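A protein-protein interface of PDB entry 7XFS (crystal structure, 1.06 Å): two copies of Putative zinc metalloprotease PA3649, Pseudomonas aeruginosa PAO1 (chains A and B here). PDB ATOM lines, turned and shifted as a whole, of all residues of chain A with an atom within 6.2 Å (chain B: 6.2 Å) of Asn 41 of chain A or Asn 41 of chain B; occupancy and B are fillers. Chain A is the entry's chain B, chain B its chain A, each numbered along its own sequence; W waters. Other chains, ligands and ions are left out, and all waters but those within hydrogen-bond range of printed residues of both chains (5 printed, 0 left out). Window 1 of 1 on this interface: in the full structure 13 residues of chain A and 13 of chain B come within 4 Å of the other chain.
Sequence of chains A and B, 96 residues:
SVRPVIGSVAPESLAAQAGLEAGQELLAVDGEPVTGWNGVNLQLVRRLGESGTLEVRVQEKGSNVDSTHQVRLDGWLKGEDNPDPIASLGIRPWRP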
ATOM      1  N   GLY A  36      22.805  -1.356  12.991  1.00  0.00           N
ATOM      2  CA  GLY A  36      24.008  -0.950  12.301  1.00  0.00           C
ATOM      3  C   GLY A  36      23.872   0.495  11.896  1.00  0.00           C
ATOM      4  O   GLY A  36      22.768   1.049  11.854  1.00  0.00           O
ATOM      5  N   TRP A  37      25.012   1.114  11.593  1.00  0.00           N
ATOM      6  CA  TRP A  37      24.986   2.511  11.182  1.00  0.00           C
ATOM      7  C   TRP A  37      24.259   2.704   9.863  1.00  0.00           C
ATOM      8  O   TRP A  37      23.686   3.770   9.640  1.00  0.00           O
ATOM      9  CB  TRP A  37      26.411   3.056  11.110  1.00  0.00           C
ATOM     10  CG  TRP A  37      26.990   3.269  12.487  1.00  0.00           C
ATOM     11  CD1 TRP A  37      27.988   2.550  13.073  1.00  0.00           C
ATOM     12  CD2 TRP A  37      26.575   4.239  13.455  1.00  0.00           C
ATOM     13  NE1 TRP A  37      28.227   3.021  14.340  1.00  0.00           N
ATOM     14  CE2 TRP A  37      27.372   4.059  14.599  1.00  0.00           C
ATOM     15  CE3 TRP A  37      25.607   5.237  13.462  1.00  0.00           C
ATOM     16  CZ2 TRP A  37      27.227   4.850  15.736  1.00  0.00           C
ATOM     17  CZ3 TRP A  37      25.475   6.037  14.581  1.00  0.00           C
ATOM     18  CH2 TRP A  37      26.271   5.830  15.711  1.00  0.00           C
ATOM     19  N   ASN A  38      24.245   1.699   8.985  1.00  0.00           N
ATOM     20  CA  ASN A  38      23.510   1.854   7.733  1.00  0.00           C
ATOM     21  C   ASN A  38      22.011   2.000   7.991  1.00  0.00           C
ATOM     22  O   ASN A  38      21.342   2.827   7.367  1.00  0.00           O
ATOM     23  CB  ASN A  38      23.807   0.686   6.800  1.00  0.00           C
ATOM     24  CG  ASN A  38      25.223   0.706   6.271  1.00  0.00           C
ATOM     25  OD1 ASN A  38      25.913   1.717   6.344  1.00  0.00           O
ATOM     26  ND2 ASN A  38      25.676  -0.419   5.763  1.00  0.00           N
ATOM     27  N   GLY A  39      21.481   1.208   8.919  1.00  0.00           N
ATOM     28  CA  GLY A  39      20.090   1.339   9.303  1.00  0.00           C
ATOM     29  C   GLY A  39      19.818   2.631  10.045  1.00  0.00           C
ATOM     30  O   GLY A  39      18.754   3.230   9.890  1.00  0.00           O
ATOM     31  N   VAL A  40      20.761   3.072  10.871  1.00  0.00           N
ATOM     32  CA  VAL A  40      20.641   4.389  11.482  1.00  0.00           C
ATOM     33  C   VAL A  40      20.464   5.443  10.400  1.00  0.00           C
ATOM     34  O   VAL A  40      19.581   6.310  10.480  1.00  0.00           O
ATOM     35  CB  VAL A  40      21.858   4.699  12.370  1.00  0.00           C
ATOM     36  CG1 VAL A  40      21.848   6.182  12.790  1.00  0.00           C
ATOM     37  CG2 VAL A  40      21.899   3.811  13.588  1.00  0.00           C
ATOM     38  N   ASN A  41      21.324   5.407   9.386  1.00  0.00           N
ATOM     39  CA  ASN A  41      21.266   6.410   8.340  1.00  0.00           C
ATOM     40  C   ASN A  41      19.910   6.443   7.643  1.00  0.00           C
ATOM     41  O   ASN A  41      19.396   7.514   7.335  1.00  0.00           O
ATOM     42  CB  ASN A  41      22.397   6.209   7.347  1.00  0.00           C
ATOM     43  CG  ASN A  41      22.675   7.470   6.582  1.00  0.00           C
ATOM     44  OD1 ASN A  41      22.823   8.528   7.175  1.00  0.00           O
ATOM     45  ND2 ASN A  41      22.708   7.378   5.278  1.00  0.00           N
ATOM     46  N   LEU A  42      19.312   5.280   7.390  1.00  0.00           N
ATOM     47  CA  LEU A  42      17.994   5.270   6.758  1.00  0.00           C
ATOM     48  C   LEU A  42      16.972   6.006   7.613  1.00  0.00           C
ATOM     49  O   LEU A  42      16.134   6.743   7.084  1.00  0.00           O
ATOM     50  CB  LEU A  42      17.502   3.851   6.509  1.00  0.00           C
ATOM     51  CG  LEU A  42      18.296   3.026   5.504  1.00  0.00           C
ATOM     52  CD1 LEU A  42      17.629   1.668   5.352  1.00  0.00           C
ATOM     53  CD2 LEU A  42      18.427   3.721   4.163  1.00  0.00           C
ATOM     54  N   GLN A  43      17.007   5.818   8.930  1.00  0.00           N
ATOM     55  CA  GLN A  43      16.074   6.543   9.790  1.00  0.00           C
ATOM     56  C   GLN A  43      16.373   8.041   9.781  1.00  0.00           C
ATOM     57  O   GLN A  43      15.452   8.866   9.779  1.00  0.00           O
ATOM     58  CB  GLN A  43      16.118   5.986  11.211  1.00  0.00           C
ATOM     59  CG  GLN A  43      15.403   4.671  11.368  1.00  0.00           C
ATOM     60  CD  GLN A  43      13.924   4.818  11.082  1.00  0.00           C
ATOM     61  OE1 GLN A  43      13.490   4.679   9.947  1.00  0.00           O
ATOM     62  NE2 GLN A  43      13.143   5.110  12.105  1.00  0.00           N
ATOM     63  N   LEU A  44      17.653   8.416   9.778  1.00  0.00           N
ATOM     64  CA  LEU A  44      18.002   9.836   9.769  1.00  0.00           C
ATOM     65  C   LEU A  44      17.538  10.528   8.498  1.00  0.00           C
ATOM     66  O   LEU A  44      17.050  11.657   8.548  1.00  0.00           O
ATOM     67  CB  LEU A  44      19.516  10.010   9.938  1.00  0.00           C
ATOM     68  CG  LEU A  44      20.108   9.516  11.248  1.00  0.00           C
ATOM     69  CD1 LEU A  44      21.607   9.784  11.273  1.00  0.00           C
ATOM     70  CD2 LEU A  44      19.438  10.148  12.459  1.00  0.00           C
ATOM     71  N   VAL A  45      17.680   9.868   7.349  1.00  0.00           N
ATOM     72  CA  VAL A  45      17.294  10.485   6.084  1.00  0.00           C
ATOM     73  C   VAL A  45      15.832  10.900   6.097  1.00  0.00           C
ATOM     74  O   VAL A  45      15.456  11.910   5.498  1.00  0.00           O
ATOM     75  CB  VAL A  45      17.642   9.520   4.933  1.00  0.00           C
ATOM     76  CG1 VAL A  45      16.895   9.866   3.650  1.00  0.00           C
ATOM     77  CG2 VAL A  45      19.156   9.506   4.743  1.00  0.00           C
ATOM     78  N   ARG A  46      14.984  10.132   6.778  1.00  0.00           N
ATOM     79  CA  ARG A  46      13.558  10.427   6.810  1.00  0.00           C
ATOM     80  C   ARG A  46      13.249  11.761   7.458  1.00  0.00           C
ATOM     81  O   ARG A  46      12.149  12.282   7.258  1.00  0.00           O
ATOM     82  CB  ARG A  46      12.795   9.317   7.535  1.00  0.00           C
ATOM     83  CG  ARG A  46      12.953   7.969   6.886  1.00  0.00           C
ATOM     84  CD  ARG A  46      12.417   6.840   7.716  1.00  0.00           C
ATOM     85  NE  ARG A  46      10.971   6.914   7.834  1.00  0.00           N
ATOM     86  CZ  ARG A  46      10.217   5.954   8.336  1.00  0.00           C
ATOM     87  NH1 ARG A  46      10.754   4.884   8.884  1.00  0.00           N
ATOM     88  NH2 ARG A  46       8.894   6.068   8.279  1.00  0.00           N
ATOM     89  N   ASP A  84      25.590  14.640   5.229  1.00  0.00           N
ATOM     90  CA  ASP A  84      26.196  13.485   5.892  1.00  0.00           C
ATOM     91  C   ASP A  84      25.460  13.393   7.230  1.00  0.00           C
ATOM     92  O   ASP A  84      25.874  14.026   8.205  1.00  0.00           O
ATOM     93  CB  ASP A  84      27.695  13.667   6.090  1.00  0.00           C
ATOM     94  CG  ASP A  84      28.369  12.454   6.733  1.00  0.00           C
ATOM     95  OD1 ASP A  84      27.691  11.697   7.479  1.00  0.00           O
ATOM     96  OD2 ASP A  84      29.594  12.304   6.555  1.00  0.00           O
ATOM     97  N   PRO A  85      24.359  12.653   7.293  1.00  0.00           N
ATOM     98  CA  PRO A  85      23.503  12.766   8.489  1.00  0.00           C
ATOM     99  C   PRO A  85      24.187  12.416   9.796  1.00  0.00           C
ATOM    100  O   PRO A  85      24.048  13.161  10.762  1.00  0.00           O
ATOM    101  CB  PRO A  85      22.321  11.858   8.157  1.00  0.00           C
ATOM    102  CG  PRO A  85      22.231  11.937   6.624  1.00  0.00           C
ATOM    103  CD  PRO A  85      23.677  11.958   6.188  1.00  0.00           C
ATOM    104  N   ILE A  86      24.908  11.303   9.877  1.00  0.00           N
ATOM    105  CA  ILE A  86      25.507  10.911  11.151  1.00  0.00           C
ATOM    106  C   ILE A  86      26.544  11.945  11.576  1.00  0.00           C
ATOM    107  O   ILE A  86      26.574  12.396  12.725  1.00  0.00           O
ATOM    108  CB  ILE A  86      26.110   9.496  11.046  1.00  0.00           C
ATOM    109  CG1 ILE A  86      25.021   8.448  10.799  1.00  0.00           C
ATOM    110  CG2 ILE A  86      26.943   9.167  12.278  1.00  0.00           C
ATOM    111  CD1 ILE A  86      25.542   7.104  10.328  1.00  0.00           C
ATOM    112  N   GLY B  36      27.511  15.224  -5.498  1.00  0.00           N
ATOM    113  CA  GLY B  36      28.366  14.549  -4.545  1.00  0.00           C
ATOM    114  C   GLY B  36      27.799  13.186  -4.237  1.00  0.00           C
ATOM    115  O   GLY B  36      26.632  12.905  -4.522  1.00  0.00           O
ATOM    116  N   TRP B  37      28.642  12.328  -3.660  1.00  0.00           N
ATOM    117  CA  TRP B  37      28.212  10.970  -3.339  1.00  0.00           C
ATOM    118  C   TRP B  37      27.126  10.954  -2.275  1.00  0.00           C
ATOM    119  O   TRP B  37      26.294  10.045  -2.269  1.00  0.00           O
ATOM    120  CB  TRP B  37      29.417  10.105  -2.930  1.00  0.00           C
ATOM    121  CG  TRP B  37      30.211   9.671  -4.125  1.00  0.00           C
ATOM    122  CD1 TRP B  37      31.445  10.101  -4.508  1.00  0.00           C
ATOM    123  CD2 TRP B  37      29.796   8.727  -5.114  1.00  0.00           C
ATOM    124  NE1 TRP B  37      31.819   9.482  -5.681  1.00  0.00           N
ATOM    125  CE2 TRP B  37      30.821   8.632  -6.068  1.00  0.00           C
ATOM    126  CE3 TRP B  37      28.661   7.944  -5.281  1.00  0.00           C
ATOM    127  CZ2 TRP B  37      30.728   7.792  -7.178  1.00  0.00           C
ATOM    128  CZ3 TRP B  37      28.582   7.103  -6.387  1.00  0.00           C
ATOM    129  CH2 TRP B  37      29.593   7.050  -7.322  1.00  0.00           C
ATOM    130  N   ASN B  38      27.096  11.943  -1.382  1.00  0.00           N
ATOM    131  CA  ASN B  38      26.031  11.966  -0.386  1.00  0.00           C
ATOM    132  C   ASN B  38      24.672  12.176  -1.040  1.00  0.00           C
ATOM    133  O   ASN B  38      23.689  11.541  -0.648  1.00  0.00           O
ATOM    134  CB  ASN B  38      26.291  13.030   0.676  1.00  0.00           C
ATOM    135  CG  ASN B  38      27.469  12.695   1.559  1.00  0.00           C
ATOM    136  OD1 ASN B  38      27.912  11.549   1.609  1.00  0.00           O
ATOM    137  ND2 ASN B  38      28.000  13.695   2.242  1.00  0.00           N
ATOM    138  N   GLY B  39      24.601  13.045  -2.047  1.00  0.00           N
ATOM    139  CA  GLY B  39      23.355  13.210  -2.773  1.00  0.00           C
ATOM    140  C   GLY B  39      23.012  12.000  -3.616  1.00  0.00           C
ATOM    141  O   GLY B  39      21.834  11.668  -3.782  1.00  0.00           O
ATOM    142  N   VAL B  40      24.022  11.334  -4.178  1.00  0.00           N
ATOM    143  CA  VAL B  40      23.783  10.061  -4.846  1.00  0.00           C
ATOM    144  C   VAL B  40      23.094   9.102  -3.886  1.00  0.00           C
ATOM    145  O   VAL B  40      22.117   8.439  -4.250  1.00  0.00           O
ATOM    146  CB  VAL B  40      25.094   9.462  -5.378  1.00  0.00           C
ATOM    147  CG1 VAL B  40      24.872   8.008  -5.821  1.00  0.00           C
ATOM    148  CG2 VAL B  40      25.676  10.307  -6.485  1.00  0.00           C
ATOM    149  N   ASN B  41      23.610   8.993  -2.666  1.00  0.00           N
ATOM    150  CA  ASN B  41      23.042   8.044  -1.720  1.00  0.00           C
ATOM    151  C   ASN B  41      21.575   8.331  -1.456  1.00  0.00           C
ATOM    152  O   ASN B  41      20.767   7.400  -1.366  1.00  0.00           O
ATOM    153  CB  ASN B  41      23.828   8.029  -0.416  1.00  0.00           C
ATOM    154  CG  ASN B  41      23.567   6.779   0.352  1.00  0.00           C
ATOM    155  OD1 ASN B  41      23.656   5.683  -0.184  1.00  0.00           O
ATOM    156  ND2 ASN B  41      23.171   6.934   1.593  1.00  0.00           N
ATOM    157  N   LEU B  42      21.191   9.605  -1.340  1.00  0.00           N
ATOM    158  CA  LEU B  42      19.781   9.914  -1.116  1.00  0.00           C
ATOM    159  C   LEU B  42      18.911   9.390  -2.251  1.00  0.00           C
ATOM    160  O   LEU B  42      17.799   8.912  -2.019  1.00  0.00           O
ATOM    161  CB  LEU B  42      19.572  11.422  -0.976  1.00  0.00           C
ATOM    162  CG  LEU B  42      20.228  12.110   0.210  1.00  0.00           C
ATOM    163  CD1 LEU B  42      19.860  13.583   0.218  1.00  0.00           C
ATOM    164  CD2 LEU B  42      19.814  11.451   1.513  1.00  0.00           C
ATOM    165  N   GLN B  43      19.383   9.503  -3.492  1.00  0.00           N
ATOM    166  CA  GLN B  43      18.610   8.971  -4.608  1.00  0.00           C
ATOM    167  C   GLN B  43      18.566   7.444  -4.582  1.00  0.00           C
ATOM    168  O   GLN B  43      17.525   6.844  -4.876  1.00  0.00           O
ATOM    169  CB  GLN B  43      19.171   9.463  -5.942  1.00  0.00           C
ATOM    170  CG  GLN B  43      18.837  10.883  -6.246  1.00  0.00           C
ATOM    171  CD  GLN B  43      17.336  11.048  -6.425  1.00  0.00           C
ATOM    172  OE1 GLN B  43      16.616  11.336  -5.480  1.00  0.00           O
ATOM    173  NE2 GLN B  43      16.851  10.793  -7.623  1.00  0.00           N
ATOM    174  N   LEU B  44      19.679   6.789  -4.221  1.00  0.00           N
ATOM    175  CA  LEU B  44      19.695   5.330  -4.173  1.00  0.00           C
ATOM    176  C   LEU B  44      18.725   4.784  -3.142  1.00  0.00           C
ATOM    177  O   LEU B  44      18.044   3.793  -3.398  1.00  0.00           O
ATOM    178  CB  LEU B  44      21.109   4.817  -3.904  1.00  0.00           C
ATOM    179  CG  LEU B  44      22.149   5.138  -4.958  1.00  0.00           C
ATOM    180  CD1 LEU B  44      23.491   4.544  -4.534  1.00  0.00           C
ATOM    181  CD2 LEU B  44      21.735   4.619  -6.328  1.00  0.00           C
ATOM    182  N   VAL B  45      18.661   5.416  -1.965  1.00  0.00           N
ATOM    183  CA  VAL B  45      17.808   4.921  -0.890  1.00  0.00           C
ATOM    184  C   VAL B  45      16.361   4.810  -1.334  1.00  0.00           C
ATOM    185  O   VAL B  45      15.634   3.911  -0.883  1.00  0.00           O
ATOM    186  CB  VAL B  45      17.978   5.826   0.351  1.00  0.00           C
ATOM    187  CG1 VAL B  45      16.810   5.675   1.313  1.00  0.00           C
ATOM    188  CG2 VAL B  45      19.322   5.515   1.026  1.00  0.00           C
ATOM    189  N   ARG B  46      15.921   5.710  -2.210  1.00  0.00           N
ATOM    190  CA  ARG B  46      14.537   5.726  -2.659  1.00  0.00           C
ATOM    191  C   ARG B  46      14.147   4.468  -3.405  1.00  0.00           C
ATOM    192  O   ARG B  46      12.951   4.189  -3.528  1.00  0.00           O
ATOM    193  CB  ARG B  46      14.288   6.930  -3.565  1.00  0.00           C
ATOM    194  CG  ARG B  46      14.569   8.259  -2.892  1.00  0.00           C
ATOM    195  CD  ARG B  46      14.576   9.413  -3.856  1.00  0.00           C
ATOM    196  NE  ARG B  46      13.232   9.670  -4.350  1.00  0.00           N
ATOM    197  CZ  ARG B  46      12.866  10.761  -4.995  1.00  0.00           C
ATOM    198  NH1 ARG B  46      13.745  11.698  -5.324  1.00  0.00           N
ATOM    199  NH2 ARG B  46      11.585  10.926  -5.296  1.00  0.00           N
ATOM    200  N   ASP B  84      24.113  -0.926   2.255  1.00  0.00           N
ATOM    201  CA  ASP B  84      25.154   0.004   1.827  1.00  0.00           C
ATOM    202  C   ASP B  84      24.912   0.232   0.349  1.00  0.00           C
ATOM    203  O   ASP B  84      25.410  -0.525  -0.498  1.00  0.00           O
ATOM    204  CB  ASP B  84      26.548  -0.562   2.073  1.00  0.00           C
ATOM    205  CG  ASP B  84      27.650   0.438   1.737  1.00  0.00           C
ATOM    206  OD1 ASP B  84      27.427   1.316   0.858  1.00  0.00           O
ATOM    207  OD2 ASP B  84      28.764   0.305   2.295  1.00  0.00           O
ATOM    208  N   PRO B  85      24.112   1.226  -0.012  1.00  0.00           N
ATOM    209  CA  PRO B  85      23.626   1.275  -1.394  1.00  0.00           C
ATOM    210  C   PRO B  85      24.719   1.372  -2.439  1.00  0.00           C
ATOM    211  O   PRO B  85      24.703   0.606  -3.408  1.00  0.00           O
ATOM    212  CB  PRO B  85      22.673   2.472  -1.382  1.00  0.00           C
ATOM    213  CG  PRO B  85      22.188   2.540   0.054  1.00  0.00           C
ATOM    214  CD  PRO B  85      23.399   2.174   0.866  1.00  0.00           C
ATOM    215  N   ILE B  86      25.668   2.297  -2.286  1.00  0.00           N
ATOM    216  CA  ILE B  86      26.690   2.460  -3.315  1.00  0.00           C
ATOM    217  C   ILE B  86      27.540   1.193  -3.435  1.00  0.00           C
ATOM    218  O   ILE B  86      27.818   0.704  -4.540  1.00  0.00           O
ATOM    219  CB  ILE B  86      27.552   3.713  -3.033  1.00  0.00           C
ATOM    220  CG1 ILE B  86      26.722   5.014  -2.972  1.00  0.00           C
ATOM    221  CG2 ILE B  86      28.644   3.854  -4.076  1.00  0.00           C
ATOM    222  CD1 ILE B  86      27.428   6.222  -2.292  1.00  0.00           C
HETATM  223  O   HOH W   1      23.595   9.302   3.287  1.00  0.00           O
HETATM  224  O   HOH W   2      30.430  13.372   3.859  1.00  0.00           O
HETATM  225  O   HOH W   3      28.540  -0.509   5.081  1.00  0.00           O
HETATM  226  O   HOH W   4      22.980   4.926   3.721  1.00  0.00           O
HETATM  227  O   HOH W   5      28.271  10.649   4.156  1.00  0.00           O
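Water W5 bridges the side-chain amide oxygen of Asn 38 of chain B (2.7 Å) and the side-chain carboxylate of Asp 84 of chain A (3.2 Å).
Water W1 bridges the side-chain amide nitrogen of Asn 41 of chain A (2.9 Å) and the side-chain amide nitrogen of Asn 41 of chain B (2.9 Å).
Water W3 lies within hydrogen-bond range of OD2 of Asp 84 of chain B and ND2 of Asn 38 of chain A.
Water W4 bridges ND2 of Asn 41 of chain A and ND2 of Asn 41 of chain B.
Water W2 bridges ND2 of Asn 38 of chain B (2.9 Å) and OD2 of Asp 84 of chain A (3.0 Å).
Of the 14 printed residues of chain A, 5 touch a printed residue of chain B.
Printed residues of chain A that touch a printed residue of chain B: Asn 38, Asn 41, Leu 42, Val 45 and Asp 84.
Hydrophobic or aromatic side chains of chain A that line the printed part of chain B: Leu 42 and Val 45.
Along chain A the printed residues that touch a printed residue of chain B span positions 38 to 84.
Among the printed residues, 5 pairs touch across the chains.
Asn 38 of chain A touches Asp 84 of chain B, and with the chains exchanged Asp 84 of chain A touches Asn 38 of chain B.
Asn 41 of chain B touches its own counterpart, Asn 41 of chain A.
Leu 42 of chain A touches Val 45 of chain B, and with the chains exchanged Val 45 of chain A touches Leu 42 of chain B.
14 positions are printed for both chains.
Among the printed residues, merely in contact across the chains: Asn 38 of chain A with Asp 84 of chain B, Asn 41 of chain A with Asn 41 of chain B, Leu 42 of chain A with Val 45 of chain B, Val 45 of chain A with Leu 42 of chain B and Asp 84 of chain A with Asn 38 of chain B.
Of the printed residues of chain B, Asn 38 of chain A touches Asp 84 (3.8 Å).
Leu 44 of chain A touches none of the printed residues of chain B.
Of the printed residues of chain B, Val 45 of chain A touches Leu 42 (3.8 Å).
Printed residues of chain B within 4 Å of Asp 84 of chain A: Asn 38.
Of chain A, only Asn 41 comes within 4 Å of Asn 41 of chain B.
Printed residues of chain A within 4 Å of Leu 42 of chain B: Val 45.
Gln 43 of chain B touches none of the printed residues of chain A.
Of the printed residues of chain A, Val 45 of chain B touches Leu 42 (3.7 Å).
The nearest residue of chain A that does not touch Asn 41 of chain B is Val 45 of chain A (5.7 Å).
The nearest printed residue of chain A that does not touch Asp 84 of chain B is Gly 39 of chain A (7.5 Å).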
